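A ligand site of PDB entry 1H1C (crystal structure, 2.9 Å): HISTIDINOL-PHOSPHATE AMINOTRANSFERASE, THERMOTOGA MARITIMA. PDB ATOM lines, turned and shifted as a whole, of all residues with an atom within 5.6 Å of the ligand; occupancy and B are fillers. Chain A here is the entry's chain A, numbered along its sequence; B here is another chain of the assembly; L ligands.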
ATOM      1  N   LEU A  26     -35.493  11.090 -18.972  1.00  0.00           N
ATOM      2  CA  LEU A  26     -34.294  11.711 -18.425  1.00  0.00           C
ATOM      3  C   LEU A  26     -33.014  10.888 -18.317  1.00  0.00           C
ATOM      4  O   LEU A  26     -32.116  11.252 -17.552  1.00  0.00           O
ATOM      5  CB  LEU A  26     -34.601  12.294 -17.038  1.00  0.00           C
ATOM      6  CG  LEU A  26     -35.353  13.620 -16.886  1.00  0.00           C
ATOM      7  CD1 LEU A  26     -35.309  14.043 -15.419  1.00  0.00           C
ATOM      8  CD2 LEU A  26     -34.717  14.688 -17.739  1.00  0.00           C
ATOM      9  N   ASN A  27     -32.910   9.802 -19.087  1.00  0.00           N
ATOM     10  CA  ASN A  27     -31.715   8.960 -19.031  1.00  0.00           C
ATOM     11  C   ASN A  27     -31.320   8.566 -17.611  1.00  0.00           C
ATOM     12  O   ASN A  27     -30.156   8.642 -17.233  1.00  0.00           O
ATOM     13  CB  ASN A  27     -30.528   9.673 -19.683  1.00  0.00           C
ATOM     14  CG  ASN A  27     -30.729   9.867 -21.154  1.00  0.00           C
ATOM     15  OD1 ASN A  27     -30.069  10.687 -21.788  1.00  0.00           O
ATOM     16  ND2 ASN A  27     -31.649   9.101 -21.731  1.00  0.00           N
ATOM     17  N   ASN A  83     -20.936  19.623  -7.847  1.00  0.00           N
ATOM     18  CA  ASN A  83     -22.310  19.301  -7.410  1.00  0.00           C
ATOM     19  C   ASN A  83     -23.089  18.836  -8.627  1.00  0.00           C
ATOM     20  O   ASN A  83     -24.026  19.499  -9.100  1.00  0.00           O
ATOM     21  CB  ASN A  83     -22.974  20.541  -6.817  1.00  0.00           C
ATOM     22  CG  ASN A  83     -24.394  20.272  -6.334  1.00  0.00           C
ATOM     23  OD1 ASN A  83     -24.626  19.475  -5.435  1.00  0.00           O
ATOM     24  ND2 ASN A  83     -25.344  20.922  -6.960  1.00  0.00           N
ATOM     25  N   GLY A  84     -22.688  17.658  -9.121  1.00  0.00           N
ATOM     26  CA  GLY A  84     -23.280  17.079 -10.307  1.00  0.00           C
ATOM     27  C   GLY A  84     -22.449  17.574 -11.482  1.00  0.00           C
ATOM     28  O   GLY A  84     -21.737  18.582 -11.359  1.00  0.00           O
ATOM     29  N   ALA A  85     -22.486  16.854 -12.593  1.00  0.00           N
ATOM     30  CA  ALA A  85     -21.752  17.298 -13.771  1.00  0.00           C
ATOM     31  C   ALA A  85     -22.331  18.670 -14.131  1.00  0.00           C
ATOM     32  O   ALA A  85     -21.631  19.540 -14.668  1.00  0.00           O
ATOM     33  CB  ALA A  85     -21.946  16.323 -14.908  1.00  0.00           C
ATOM     34  N   ASP A  86     -23.598  18.881 -13.819  1.00  0.00           N
ATOM     35  CA  ASP A  86     -24.226  20.158 -14.097  1.00  0.00           C
ATOM     36  C   ASP A  86     -23.455  21.315 -13.459  1.00  0.00           C
ATOM     37  O   ASP A  86     -23.144  22.280 -14.153  1.00  0.00           O
ATOM     38  CB  ASP A  86     -25.674  20.154 -13.612  1.00  0.00           C
ATOM     39  CG  ASP A  86     -26.633  19.643 -14.660  1.00  0.00           C
ATOM     40  OD1 ASP A  86     -26.196  18.805 -15.473  1.00  0.00           O
ATOM     41  OD2 ASP A  86     -27.803  20.072 -14.683  1.00  0.00           O
ATOM     42  N   GLU A  87     -23.134  21.222 -12.172  1.00  0.00           N
ATOM     43  CA  GLU A  87     -22.418  22.319 -11.542  1.00  0.00           C
ATOM     44  C   GLU A  87     -21.088  22.565 -12.258  1.00  0.00           C
ATOM     45  O   GLU A  87     -20.648  23.702 -12.347  1.00  0.00           O
ATOM     46  CB  GLU A  87     -22.170  22.074 -10.026  1.00  0.00           C
ATOM     47  CG  GLU A  87     -21.522  23.291  -9.331  1.00  0.00           C
ATOM     48  CD  GLU A  87     -20.880  22.986  -7.959  1.00  0.00           C
ATOM     49  OE1 GLU A  87     -19.977  22.137  -7.868  1.00  0.00           O
ATOM     50  OE2 GLU A  87     -21.262  23.621  -6.972  1.00  0.00           O
ATOM     51  N   ILE A  89     -20.422  22.186 -15.491  1.00  0.00           N
ATOM     52  CA  ILE A  89     -20.799  22.958 -16.678  1.00  0.00           C
ATOM     53  C   ILE A  89     -21.087  24.391 -16.275  1.00  0.00           C
ATOM     54  O   ILE A  89     -20.614  25.354 -16.888  1.00  0.00           O
ATOM     55  CB  ILE A  89     -22.108  22.480 -17.285  1.00  0.00           C
ATOM     56  CG1 ILE A  89     -22.117  20.954 -17.425  1.00  0.00           C
ATOM     57  CG2 ILE A  89     -22.315  23.228 -18.583  1.00  0.00           C
ATOM     58  CD1 ILE A  89     -21.183  20.418 -18.472  1.00  0.00           C
ATOM     59  N   TYR A 106     -26.745  18.741 -25.380  1.00  0.00           N
ATOM     60  CA  TYR A 106     -27.281  18.766 -24.025  1.00  0.00           C
ATOM     61  C   TYR A 106     -28.032  20.078 -23.844  1.00  0.00           C
ATOM     62  O   TYR A 106     -27.406  21.133 -23.740  1.00  0.00           O
ATOM     63  CB  TYR A 106     -26.136  18.638 -23.030  1.00  0.00           C
ATOM     64  CG  TYR A 106     -26.570  18.591 -21.603  1.00  0.00           C
ATOM     65  CD1 TYR A 106     -27.627  17.774 -21.189  1.00  0.00           C
ATOM     66  CD2 TYR A 106     -25.926  19.367 -20.647  1.00  0.00           C
ATOM     67  CE1 TYR A 106     -28.026  17.729 -19.859  1.00  0.00           C
ATOM     68  CE2 TYR A 106     -26.303  19.322 -19.314  1.00  0.00           C
ATOM     69  CZ  TYR A 106     -27.358  18.505 -18.921  1.00  0.00           C
ATOM     70  OH  TYR A 106     -27.694  18.472 -17.592  1.00  0.00           O
ATOM     71  N   TYR A 109     -27.000  23.226 -21.642  1.00  0.00           N
ATOM     72  CA  TYR A 109     -25.896  24.117 -22.018  1.00  0.00           C
ATOM     73  C   TYR A 109     -26.471  25.499 -22.266  1.00  0.00           C
ATOM     74  O   TYR A 109     -26.093  26.479 -21.631  1.00  0.00           O
ATOM     75  CB  TYR A 109     -25.202  23.639 -23.304  1.00  0.00           C
ATOM     76  CG  TYR A 109     -24.412  22.388 -23.127  1.00  0.00           C
ATOM     77  CD1 TYR A 109     -23.814  22.097 -21.901  1.00  0.00           C
ATOM     78  CD2 TYR A 109     -24.208  21.512 -24.181  1.00  0.00           C
ATOM     79  CE1 TYR A 109     -23.052  20.963 -21.724  1.00  0.00           C
ATOM     80  CE2 TYR A 109     -23.441  20.365 -24.014  1.00  0.00           C
ATOM     81  CZ  TYR A 109     -22.866  20.097 -22.780  1.00  0.00           C
ATOM     82  OH  TYR A 109     -22.106  18.963 -22.593  1.00  0.00           O
ATOM     83  N   PRO A 145     -20.510  17.033 -25.790  1.00  0.00           N
ATOM     84  CA  PRO A 145     -20.814  15.820 -25.031  1.00  0.00           C
ATOM     85  C   PRO A 145     -20.689  14.561 -25.893  1.00  0.00           C
ATOM     86  O   PRO A 145     -21.516  14.293 -26.748  1.00  0.00           O
ATOM     87  CB  PRO A 145     -22.245  16.065 -24.627  1.00  0.00           C
ATOM     88  CG  PRO A 145     -22.799  16.531 -25.914  1.00  0.00           C
ATOM     89  CD  PRO A 145     -21.757  17.624 -26.282  1.00  0.00           C
ATOM     90  N   ASN A 149     -25.733  13.926 -26.634  1.00  0.00           N
ATOM     91  CA  ASN A 149     -27.103  13.938 -26.158  1.00  0.00           C
ATOM     92  C   ASN A 149     -27.819  14.914 -27.110  1.00  0.00           C
ATOM     93  O   ASN A 149     -27.344  16.000 -27.347  1.00  0.00           O
ATOM     94  CB  ASN A 149     -27.202  14.473 -24.716  1.00  0.00           C
ATOM     95  CG  ASN A 149     -28.629  14.337 -24.140  1.00  0.00           C
ATOM     96  OD1 ASN A 149     -29.609  14.741 -24.765  1.00  0.00           O
ATOM     97  ND2 ASN A 149     -28.744  13.770 -22.969  1.00  0.00           N
ATOM     98  N   ASP A 173     -17.683  16.438 -22.562  1.00  0.00           N
ATOM     99  CA  ASP A 173     -18.696  15.958 -21.620  1.00  0.00           C
ATOM    100  C   ASP A 173     -18.962  14.486 -21.851  1.00  0.00           C
ATOM    101  O   ASP A 173     -19.775  14.118 -22.697  1.00  0.00           O
ATOM    102  CB  ASP A 173     -19.978  16.757 -21.820  1.00  0.00           C
ATOM    103  CG  ASP A 173     -21.057  16.354 -20.845  1.00  0.00           C
ATOM    104  OD1 ASP A 173     -21.145  15.157 -20.512  1.00  0.00           O
ATOM    105  OD2 ASP A 173     -21.837  17.239 -20.415  1.00  0.00           O
ATOM    106  N   ALA A 175     -20.527  12.418 -19.949  1.00  0.00           N
ATOM    107  CA  ALA A 175     -21.538  11.984 -19.016  1.00  0.00           C
ATOM    108  C   ALA A 175     -21.969  10.549 -19.327  1.00  0.00           C
ATOM    109  O   ALA A 175     -22.383   9.814 -18.439  1.00  0.00           O
ATOM    110  CB  ALA A 175     -22.740  12.919 -19.062  1.00  0.00           C
ATOM    111  N   TYR A 176     -21.838  10.151 -20.591  1.00  0.00           N
ATOM    112  CA  TYR A 176     -22.265   8.812 -20.989  1.00  0.00           C
ATOM    113  C   TYR A 176     -21.170   7.795 -21.292  1.00  0.00           C
ATOM    114  O   TYR A 176     -21.428   6.763 -21.924  1.00  0.00           O
ATOM    115  CB  TYR A 176     -23.184   8.910 -22.209  1.00  0.00           C
ATOM    116  CG  TYR A 176     -24.461   9.635 -21.886  1.00  0.00           C
ATOM    117  CD1 TYR A 176     -25.327   9.134 -20.937  1.00  0.00           C
ATOM    118  CD2 TYR A 176     -24.787  10.829 -22.511  1.00  0.00           C
ATOM    119  CE1 TYR A 176     -26.485   9.807 -20.600  1.00  0.00           C
ATOM    120  CE2 TYR A 176     -25.957  11.521 -22.186  1.00  0.00           C
ATOM    121  CZ  TYR A 176     -26.802  10.996 -21.225  1.00  0.00           C
ATOM    122  OH  TYR A 176     -27.933  11.686 -20.854  1.00  0.00           O
ATOM    123  N   ARG A 198     -17.171  13.832 -16.051  1.00  0.00           N
ATOM    124  CA  ARG A 198     -17.720  12.516 -15.739  1.00  0.00           C
ATOM    125  C   ARG A 198     -18.817  12.663 -14.702  1.00  0.00           C
ATOM    126  O   ARG A 198     -18.944  13.719 -14.087  1.00  0.00           O
ATOM    127  CB  ARG A 198     -16.634  11.611 -15.213  1.00  0.00           C
ATOM    128  CG  ARG A 198     -15.679  11.111 -16.277  1.00  0.00           C
ATOM    129  CD  ARG A 198     -16.382  10.220 -17.253  1.00  0.00           C
ATOM    130  NE  ARG A 198     -15.458   9.587 -18.172  1.00  0.00           N
ATOM    131  CZ  ARG A 198     -14.545   8.686 -17.819  1.00  0.00           C
ATOM    132  NH1 ARG A 198     -14.435   8.299 -16.565  1.00  0.00           N
ATOM    133  NH2 ARG A 198     -13.743   8.163 -18.741  1.00  0.00           N
ATOM    134  N   THR A 199     -19.575  11.602 -14.469  1.00  0.00           N
ATOM    135  CA  THR A 199     -20.673  11.688 -13.514  1.00  0.00           C
ATOM    136  C   THR A 199     -21.141  10.363 -12.950  1.00  0.00           C
ATOM    137  O   THR A 199     -21.063   9.329 -13.641  1.00  0.00           O
ATOM    138  CB  THR A 199     -21.909  12.324 -14.196  1.00  0.00           C
ATOM    139  OG1 THR A 199     -22.920  12.577 -13.216  1.00  0.00           O
ATOM    140  CG2 THR A 199     -22.482  11.347 -15.228  1.00  0.00           C
ATOM    141  N   PHE A 200     -21.652  10.387 -11.722  1.00  0.00           N
ATOM    142  CA  PHE A 200     -22.200   9.202 -11.094  1.00  0.00           C
ATOM    143  C   PHE A 200     -23.759   9.186 -11.217  1.00  0.00           C
ATOM    144  O   PHE A 200     -24.416   8.232 -10.747  1.00  0.00           O
ATOM    145  CB  PHE A 200     -21.815   9.138  -9.626  1.00  0.00           C
ATOM    146  CG  PHE A 200     -20.363   9.004  -9.369  1.00  0.00           C
ATOM    147  CD1 PHE A 200     -19.530  10.113  -9.430  1.00  0.00           C
ATOM    148  CD2 PHE A 200     -19.819   7.785  -8.979  1.00  0.00           C
ATOM    149  CE1 PHE A 200     -18.180  10.002  -9.074  1.00  0.00           C
ATOM    150  CE2 PHE A 200     -18.460   7.669  -8.622  1.00  0.00           C
ATOM    151  CZ  PHE A 200     -17.643   8.773  -8.665  1.00  0.00           C
ATOM    152  N   SER A 201     -24.339  10.199 -11.868  1.00  0.00           N
ATOM    153  CA  SER A 201     -25.790  10.231 -12.017  1.00  0.00           C
ATOM    154  C   SER A 201     -26.351   9.119 -12.880  1.00  0.00           C
ATOM    155  O   SER A 201     -27.370   8.526 -12.537  1.00  0.00           O
ATOM    156  CB  SER A 201     -26.253  11.561 -12.595  1.00  0.00           C
ATOM    157  OG  SER A 201     -26.172  12.551 -11.593  1.00  0.00           O
ATOM    158  N   LYS A 202     -25.705   8.857 -14.016  1.00  0.00           N
ATOM    159  CA  LYS A 202     -26.095   7.810 -14.967  1.00  0.00           C
ATOM    160  C   LYS A 202     -26.063   6.300 -14.778  1.00  0.00           C
ATOM    161  O   LYS A 202     -27.085   5.646 -14.609  1.00  0.00           O
ATOM    162  CB  LYS A 202     -26.237   8.488 -16.369  1.00  0.00           C
ATOM    163  CG  LYS A 202     -26.354  10.033 -16.446  1.00  0.00           C
ATOM    164  CD  LYS A 202     -27.834  10.429 -16.307  1.00  0.00           C
ATOM    165  CE  LYS A 202     -28.287  11.853 -16.731  1.00  0.00           C
ATOM    166  NZ  LYS A 202     -27.263  12.844 -17.235  1.00  0.00           N
ATOM    167  N   ALA A 207     -28.003   9.743  -9.349  1.00  0.00           N
ATOM    168  CA  ALA A 207     -28.372  11.072  -9.846  1.00  0.00           C
ATOM    169  C   ALA A 207     -28.981  11.966  -8.760  1.00  0.00           C
ATOM    170  O   ALA A 207     -28.872  13.195  -8.807  1.00  0.00           O
ATOM    171  CB  ALA A 207     -29.350  10.924 -11.019  1.00  0.00           C
ATOM    172  N   ARG A 210     -26.269  14.039  -6.761  1.00  0.00           N
ATOM    173  CA  ARG A 210     -25.465  14.975  -7.505  1.00  0.00           C
ATOM    174  C   ARG A 210     -23.983  14.866  -7.193  1.00  0.00           C
ATOM    175  O   ARG A 210     -23.507  15.459  -6.232  1.00  0.00           O
ATOM    176  CB  ARG A 210     -25.945  16.393  -7.197  1.00  0.00           C
ATOM    177  CG  ARG A 210     -27.436  16.470  -6.855  1.00  0.00           C
ATOM    178  CD  ARG A 210     -28.345  16.114  -8.015  1.00  0.00           C
ATOM    179  NE  ARG A 210     -28.044  16.922  -9.177  1.00  0.00           N
ATOM    180  CZ  ARG A 210     -27.181  16.550 -10.118  1.00  0.00           C
ATOM    181  NH1 ARG A 210     -26.574  15.391 -10.011  1.00  0.00           N
ATOM    182  NH2 ARG A 210     -26.907  17.359 -11.132  1.00  0.00           N
ATOM    183  N   VAL A 211     -23.267  14.083  -7.991  1.00  0.00           N
ATOM    184  CA  VAL A 211     -21.836  13.920  -7.787  1.00  0.00           C
ATOM    185  C   VAL A 211     -21.118  13.729  -9.124  1.00  0.00           C
ATOM    186  O   VAL A 211     -21.182  12.660  -9.733  1.00  0.00           O
ATOM    187  CB  VAL A 211     -21.551  12.733  -6.864  1.00  0.00           C
ATOM    188  CG1 VAL A 211     -20.050  12.465  -6.786  1.00  0.00           C
ATOM    189  CG2 VAL A 211     -22.105  13.026  -5.484  1.00  0.00           C
ATOM    190  N   GLY A 212     -20.443  14.785  -9.569  1.00  0.00           N
ATOM    191  CA  GLY A 212     -19.712  14.739 -10.830  1.00  0.00           C
ATOM    192  C   GLY A 212     -18.250  15.132 -10.680  1.00  0.00           C
ATOM    193  O   GLY A 212     -17.861  15.816  -9.728  1.00  0.00           O
ATOM    194  N   TYR B  53     -33.625  12.087 -10.663  1.00  0.00           N
ATOM    195  CA  TYR B  53     -33.339  13.477 -10.391  1.00  0.00           C
ATOM    196  C   TYR B  53     -34.419  14.012  -9.474  1.00  0.00           C
ATOM    197  O   TYR B  53     -35.408  14.586  -9.915  1.00  0.00           O
ATOM    198  CB  TYR B  53     -33.310  14.260 -11.689  1.00  0.00           C
ATOM    199  CG  TYR B  53     -32.028  14.092 -12.441  1.00  0.00           C
ATOM    200  CD1 TYR B  53     -30.921  14.889 -12.164  1.00  0.00           C
ATOM    201  CD2 TYR B  53     -31.891  13.109 -13.416  1.00  0.00           C
ATOM    202  CE1 TYR B  53     -29.709  14.716 -12.824  1.00  0.00           C
ATOM    203  CE2 TYR B  53     -30.682  12.927 -14.088  1.00  0.00           C
ATOM    204  CZ  TYR B  53     -29.599  13.746 -13.792  1.00  0.00           C
ATOM    205  OH  TYR B  53     -28.409  13.610 -14.485  1.00  0.00           O
HETATM  206  N1  LIG L   1     -24.185  16.483 -19.273  1.00  0.00           N
HETATM  207  C1  LIG L   1     -24.815  15.689 -20.238  1.00  0.00           C
HETATM  208  C2  LIG L   1     -24.248  15.799 -21.636  1.00  0.00           C
HETATM  209  C3  LIG L   1     -25.971  14.828 -19.767  1.00  0.00           C
HETATM  210  O1  LIG L   1     -26.518  14.081 -20.730  1.00  0.00           O
HETATM  211  C4  LIG L   1     -26.382  14.854 -18.396  1.00  0.00           C
HETATM  212  C5  LIG L   1     -27.531  13.994 -17.975  1.00  0.00           C
HETATM  213  C6  LIG L   1     -25.597  15.806 -17.449  1.00  0.00           C
HETATM  214  C7  LIG L   1     -24.527  16.575 -17.902  1.00  0.00           C
HETATM  215  C8  LIG L   1     -26.018  15.860 -15.958  1.00  0.00           C
HETATM  216  O2  LIG L   1     -25.078  15.276 -15.120  1.00  0.00           O
HETATM  217  P1  LIG L   1     -25.304  15.398 -13.512  1.00  0.00           P
HETATM  218  O3  LIG L   1     -24.155  14.682 -12.944  1.00  0.00           O
HETATM  219  O4  LIG L   1     -26.688  14.754 -13.225  1.00  0.00           O
HETATM  220  O5  LIG L   1     -25.318  16.853 -13.206  1.00  0.00           O
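An oxygen (O1) of the ligand sits at hydrogen-bond distance from the side-chain amide nitrogen (ND2) of Asn 149, at 3.2 Å. An oxygen (O1) of the ligand sits at hydrogen-bond distance from the side-chain hydroxyl of Tyr 176 (2.8 Å). The side-chain carboxylate of Asp 173 lies within hydrogen-bond range of a nitrogen (N1) of the ligand, at 2.7 Å. NH2 of Arg 210 is in salt-bridge range of O5 of the ligand (2.7 Å). NZ of Lys 202 is covalently linked to C5 of the ligand (1.4 Å). OG of Ser 201 sits at hydrogen-bond distance from O4 of the ligand (2.8 Å). O3 of the ligand sits at hydrogen-bond distance from N of Ala 85 (2.8 Å). The side-chain hydroxyl (OG1) of Thr 199 lies within hydrogen-bond range of an oxygen (O3) of the ligand. OH of Tyr 53 of chain B is in hydrogen-bond range of O4 of the ligand (2.4 Å). O5 of the ligand is in hydrogen-bond range of N of Asp 86.
The guanidinium group (NH1) of Arg 210 sits close to the backbone carbonyl oxygen (O) of Ala 207. NZ of Lys 202 sits close to OH of Tyr 53 of chain B, 3.1 Å away. OG1 of Thr 199 lies within hydrogen-bond range of N of Ser 201 (3.1 Å). O of Ser 201 lies close to N of Ala 207, at 3.5 Å. OH of Tyr 176 sits at hydrogen-bond distance from OD1 of Asn 27 (2.5 Å). OD1 of Asp 173 sits at hydrogen-bond distance from N of Ala 175 (2.9 Å). The side-chain hydroxyl (OH) of Tyr 106 sits at hydrogen-bond distance from the side-chain carboxylate (OD1) of Asp 86. The side-chain hydroxyl (OH) of Tyr 176 lies within hydrogen-bond range of the side-chain amide nitrogen (ND2) of Asn 149 (3.1 Å).
Gly 84 touches the ligand. Tyr 106 touches the ligand (OH to C6, 3.4 Å). Tyr 109 touches the ligand (OH to C2, 3.9 Å). Pro 145 touches the ligand (CB to C2, 3.6 Å). Ala 175 touches the ligand (CB to C1, 3.7 Å). Of the 25 residues printed, 15 come within 4 Å of the ligand. The nearest printed residue that does not touch the ligand is Val 211 (4.8 Å).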
